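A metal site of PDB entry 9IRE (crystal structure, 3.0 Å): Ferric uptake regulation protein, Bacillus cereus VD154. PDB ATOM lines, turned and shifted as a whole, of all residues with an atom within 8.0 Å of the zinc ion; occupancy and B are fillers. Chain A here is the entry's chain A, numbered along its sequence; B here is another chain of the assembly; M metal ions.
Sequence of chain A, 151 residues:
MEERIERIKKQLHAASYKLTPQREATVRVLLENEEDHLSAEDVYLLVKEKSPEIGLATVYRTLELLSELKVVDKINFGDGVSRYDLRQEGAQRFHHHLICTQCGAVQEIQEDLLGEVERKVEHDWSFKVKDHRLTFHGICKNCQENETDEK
The side-chain sulfur (SG) of Cys 140 sits close to the backbone NH (N) of Asn 142, 3.8 Å away. O of Ala 105 lies within hydrogen-bond range of N of Cys 100, at 2.9 Å. The backbone NH (N) of Ala 105 lies close to the side-chain sulfur (SG) of Cys 103. The side-chain amide nitrogen (NE2) of Gln 144 lies within hydrogen-bond range of the backbone carbonyl oxygen (O) of Cys 140 (3.0 Å). SG of Cys 143 sits close to NE2 of Gln 102 (2.8 Å).
Four residues have an atom within 4 Å of the zinc ion: Cys 100, Cys 103, Cys 140 and Cys 143. The nearest printed residue that does not touch the zinc ion is Gln 102 (4.5 Å).
SG of Cys 103 is bound to the zinc ion (2.2 Å). The zinc ion is bound by SG of Cys 140. The side-chain sulfur (SG) of Cys 100 is bound to the zinc ion, at 2.3 Å. The zinc ion is bound by the side-chain sulfur (SG) of Cys 143.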
ATOM      1  N   ILE A  99     -27.567   3.470 -33.477  1.00  0.00           N
ATOM      2  CA  ILE A  99     -27.466   2.252 -32.691  1.00  0.00           C
ATOM      3  C   ILE A  99     -26.827   2.601 -31.355  1.00  0.00           C
ATOM      4  O   ILE A  99     -25.934   3.463 -31.280  1.00  0.00           O
ATOM      5  CB  ILE A  99     -26.629   1.213 -33.437  1.00  0.00           C
ATOM      6  CG1 ILE A  99     -27.211   0.970 -34.825  1.00  0.00           C
ATOM      7  CG2 ILE A  99     -26.539  -0.044 -32.631  1.00  0.00           C
ATOM      8  CD1 ILE A  99     -26.281   0.234 -35.737  1.00  0.00           C
ATOM      9  N   CYS A 100     -27.299   1.961 -30.297  1.00  0.00           N
ATOM     10  CA  CYS A 100     -26.719   2.078 -28.966  1.00  0.00           C
ATOM     11  C   CYS A 100     -25.806   0.888 -28.715  1.00  0.00           C
ATOM     12  O   CYS A 100     -26.170  -0.260 -28.997  1.00  0.00           O
ATOM     13  CB  CYS A 100     -27.829   2.131 -27.920  1.00  0.00           C
ATOM     14  SG  CYS A 100     -27.212   2.601 -26.344  1.00  0.00           S
ATOM     15  N   THR A 101     -24.602   1.160 -28.229  1.00  0.00           N
ATOM     16  CA  THR A 101     -23.632   0.094 -28.017  1.00  0.00           C
ATOM     17  C   THR A 101     -23.629  -0.348 -26.568  1.00  0.00           C
ATOM     18  O   THR A 101     -22.628  -0.225 -25.861  1.00  0.00           O
ATOM     19  CB  THR A 101     -22.232   0.562 -28.408  1.00  0.00           C
ATOM     20  OG1 THR A 101     -21.891   1.709 -27.627  1.00  0.00           O
ATOM     21  CG2 THR A 101     -22.174   0.928 -29.884  1.00  0.00           C
ATOM     22  N   GLN A 102     -24.753  -0.896 -26.138  1.00  0.00           N
ATOM     23  CA  GLN A 102     -24.936  -1.249 -24.739  1.00  0.00           C
ATOM     24  C   GLN A 102     -26.339  -1.809 -24.606  1.00  0.00           C
ATOM     25  O   GLN A 102     -26.561  -3.013 -24.754  1.00  0.00           O
ATOM     26  CB  GLN A 102     -24.736  -0.020 -23.859  1.00  0.00           C
ATOM     27  CG  GLN A 102     -25.034  -0.233 -22.401  1.00  0.00           C
ATOM     28  CD  GLN A 102     -25.608   1.011 -21.779  1.00  0.00           C
ATOM     29  OE1 GLN A 102     -24.950   2.052 -21.703  1.00  0.00           O
ATOM     30  NE2 GLN A 102     -26.873   0.929 -21.350  1.00  0.00           N
ATOM     31  N   CYS A 103     -27.294  -0.895 -24.392  1.00  0.00           N
ATOM     32  CA  CYS A 103     -28.714  -1.270 -24.385  1.00  0.00           C
ATOM     33  C   CYS A 103     -29.115  -1.857 -25.740  1.00  0.00           C
ATOM     34  O   CYS A 103     -29.892  -2.823 -25.795  1.00  0.00           O
ATOM     35  CB  CYS A 103     -29.565  -0.049 -24.030  1.00  0.00           C
ATOM     36  SG  CYS A 103     -30.011   1.028 -25.416  1.00  0.00           S
ATOM     37  N   GLY A 104     -28.577  -1.303 -26.832  1.00  0.00           N
ATOM     38  CA  GLY A 104     -28.838  -1.811 -28.165  1.00  0.00           C
ATOM     39  C   GLY A 104     -30.086  -1.266 -28.844  1.00  0.00           C
ATOM     40  O   GLY A 104     -30.645  -1.954 -29.700  1.00  0.00           O
ATOM     41  N   ALA A 105     -30.541  -0.075 -28.464  1.00  0.00           N
ATOM     42  CA  ALA A 105     -31.640   0.568 -29.169  1.00  0.00           C
ATOM     43  C   ALA A 105     -31.202   0.990 -30.569  1.00  0.00           C
ATOM     44  O   ALA A 105     -30.032   1.295 -30.826  1.00  0.00           O
ATOM     45  CB  ALA A 105     -32.140   1.759 -28.379  1.00  0.00           C
ATOM     46  N   VAL A 106     -32.167   1.015 -31.488  1.00  0.00           N
ATOM     47  CA  VAL A 106     -31.925   1.412 -32.863  1.00  0.00           C
ATOM     48  C   VAL A 106     -32.987   2.432 -33.229  1.00  0.00           C
ATOM     49  O   VAL A 106     -34.181   2.162 -33.086  1.00  0.00           O
ATOM     50  CB  VAL A 106     -32.017   0.212 -33.812  1.00  0.00           C
ATOM     51  CG1 VAL A 106     -31.767   0.639 -35.212  1.00  0.00           C
ATOM     52  CG2 VAL A 106     -31.078  -0.907 -33.404  1.00  0.00           C
ATOM     53  N   GLN A 107     -32.547   3.596 -33.720  1.00  0.00           N
ATOM     54  CA  GLN A 107     -33.453   4.675 -34.104  1.00  0.00           C
ATOM     55  C   GLN A 107     -33.327   4.926 -35.598  1.00  0.00           C
ATOM     56  O   GLN A 107     -32.326   5.494 -36.061  1.00  0.00           O
ATOM     57  CB  GLN A 107     -33.146   5.957 -33.338  1.00  0.00           C
ATOM     58  CG  GLN A 107     -34.097   6.287 -32.194  1.00  0.00           C
ATOM     59  CD  GLN A 107     -33.367   7.063 -31.119  1.00  0.00           C
ATOM     60  OE1 GLN A 107     -32.517   7.888 -31.427  1.00  0.00           O
ATOM     61  NE2 GLN A 107     -33.635   6.748 -29.861  1.00  0.00           N
ATOM     62  N   GLY A 138     -23.051   4.898 -30.435  1.00  0.00           N
ATOM     63  CA  GLY A 138     -22.889   5.731 -29.267  1.00  0.00           C
ATOM     64  C   GLY A 138     -23.879   5.420 -28.170  1.00  0.00           C
ATOM     65  O   GLY A 138     -25.011   5.012 -28.439  1.00  0.00           O
ATOM     66  N   ILE A 139     -23.468   5.552 -26.918  1.00  0.00           N
ATOM     67  CA  ILE A 139     -24.377   5.230 -25.835  1.00  0.00           C
ATOM     68  C   ILE A 139     -25.503   6.263 -25.847  1.00  0.00           C
ATOM     69  O   ILE A 139     -25.257   7.482 -25.949  1.00  0.00           O
ATOM     70  CB  ILE A 139     -23.600   5.113 -24.512  1.00  0.00           C
ATOM     71  CG1 ILE A 139     -22.956   3.707 -24.422  1.00  0.00           C
ATOM     72  CG2 ILE A 139     -24.460   5.441 -23.312  1.00  0.00           C
ATOM     73  CD1 ILE A 139     -22.000   3.404 -23.223  1.00  0.00           C
ATOM     74  N   CYS A 140     -26.752   5.772 -25.849  1.00  0.00           N
ATOM     75  CA  CYS A 140     -27.907   6.600 -26.206  1.00  0.00           C
ATOM     76  C   CYS A 140     -28.410   7.480 -25.048  1.00  0.00           C
ATOM     77  O   CYS A 140     -27.896   7.463 -23.924  1.00  0.00           O
ATOM     78  CB  CYS A 140     -29.047   5.715 -26.696  1.00  0.00           C
ATOM     79  SG  CYS A 140     -29.889   4.895 -25.317  1.00  0.00           S
ATOM     80  N   LYS A 141     -29.469   8.242 -25.346  1.00  0.00           N
ATOM     81  CA  LYS A 141     -29.928   9.289 -24.447  1.00  0.00           C
ATOM     82  C   LYS A 141     -30.181   8.760 -23.060  1.00  0.00           C
ATOM     83  O   LYS A 141     -29.719   9.333 -22.074  1.00  0.00           O
ATOM     84  CB  LYS A 141     -31.216   9.932 -24.967  1.00  0.00           C
ATOM     85  CG  LYS A 141     -31.835  10.880 -23.944  1.00  0.00           C
ATOM     86  CD  LYS A 141     -33.018  11.612 -24.514  1.00  0.00           C
ATOM     87  CE  LYS A 141     -33.572  12.586 -23.503  1.00  0.00           C
ATOM     88  NZ  LYS A 141     -34.507  13.585 -24.138  1.00  0.00           N
ATOM     89  N   ASN A 142     -30.953   7.678 -22.977  1.00  0.00           N
ATOM     90  CA  ASN A 142     -31.366   7.125 -21.698  1.00  0.00           C
ATOM     91  C   ASN A 142     -30.251   6.344 -20.996  1.00  0.00           C
ATOM     92  O   ASN A 142     -30.322   6.167 -19.780  1.00  0.00           O
ATOM     93  CB  ASN A 142     -32.582   6.208 -21.894  1.00  0.00           C
ATOM     94  CG  ASN A 142     -33.892   6.929 -21.729  1.00  0.00           C
ATOM     95  OD1 ASN A 142     -34.705   6.947 -22.653  1.00  0.00           O
ATOM     96  ND2 ASN A 142     -34.108   7.518 -20.564  1.00  0.00           N
ATOM     97  N   CYS A 143     -29.230   5.866 -21.730  1.00  0.00           N
ATOM     98  CA  CYS A 143     -28.091   5.262 -21.068  1.00  0.00           C
ATOM     99  C   CYS A 143     -27.124   6.287 -20.525  1.00  0.00           C
ATOM    100  O   CYS A 143     -26.184   5.916 -19.818  1.00  0.00           O
ATOM    101  CB  CYS A 143     -27.343   4.326 -21.996  1.00  0.00           C
ATOM    102  SG  CYS A 143     -28.362   3.000 -22.569  1.00  0.00           S
ATOM    103  N   GLN A 144     -27.299   7.558 -20.838  1.00  0.00           N
ATOM    104  CA  GLN A 144     -26.550   8.588 -20.147  1.00  0.00           C
ATOM    105  C   GLN A 144     -27.095   8.811 -18.748  1.00  0.00           C
ATOM    106  O   GLN A 144     -26.326   9.126 -17.828  1.00  0.00           O
ATOM    107  CB  GLN A 144     -26.543   9.872 -20.975  1.00  0.00           C
ATOM    108  CG  GLN A 144     -25.700   9.687 -22.231  1.00  0.00           C
ATOM    109  CD  GLN A 144     -26.055  10.640 -23.340  1.00  0.00           C
ATOM    110  OE1 GLN A 144     -25.839  11.860 -23.243  1.00  0.00           O
ATOM    111  NE2 GLN A 144     -26.578  10.088 -24.429  1.00  0.00           N
ATOM    112  N   ASN A 146     -29.115   6.556 -16.884  1.00  0.00           N
ATOM    113  CA  ASN A 146     -29.278   5.374 -16.057  1.00  0.00           C
ATOM    114  C   ASN A 146     -27.955   4.749 -15.658  1.00  0.00           C
ATOM    115  O   ASN A 146     -27.941   3.789 -14.873  1.00  0.00           O
ATOM    116  CB  ASN A 146     -30.152   4.327 -16.771  1.00  0.00           C
ATOM    117  CG  ASN A 146     -31.560   4.817 -16.953  1.00  0.00           C
ATOM    118  OD1 ASN A 146     -32.004   5.736 -16.263  1.00  0.00           O
ATOM    119  ND2 ASN A 146     -32.292   4.202 -17.869  1.00  0.00           N
ATOM    120  N   PHE B 127     -27.968  12.123 -28.151  1.00  0.00           N
ATOM    121  CA  PHE B 127     -27.206  10.924 -28.410  1.00  0.00           C
ATOM    122  C   PHE B 127     -25.740  11.287 -28.296  1.00  0.00           C
ATOM    123  O   PHE B 127     -25.321  12.382 -28.702  1.00  0.00           O
ATOM    124  CB  PHE B 127     -27.521  10.404 -29.808  1.00  0.00           C
ATOM    125  CG  PHE B 127     -27.248   8.954 -30.009  1.00  0.00           C
ATOM    126  CD1 PHE B 127     -28.146   8.007 -29.584  1.00  0.00           C
ATOM    127  CD2 PHE B 127     -26.120   8.537 -30.689  1.00  0.00           C
ATOM    128  CE1 PHE B 127     -27.903   6.657 -29.814  1.00  0.00           C
ATOM    129  CE2 PHE B 127     -25.895   7.201 -30.922  1.00  0.00           C
ATOM    130  CZ  PHE B 127     -26.775   6.264 -30.488  1.00  0.00           C
HETATM  131 ZN    ZN M   1     -28.911   2.893 -24.844  1.00  0.00          ZN
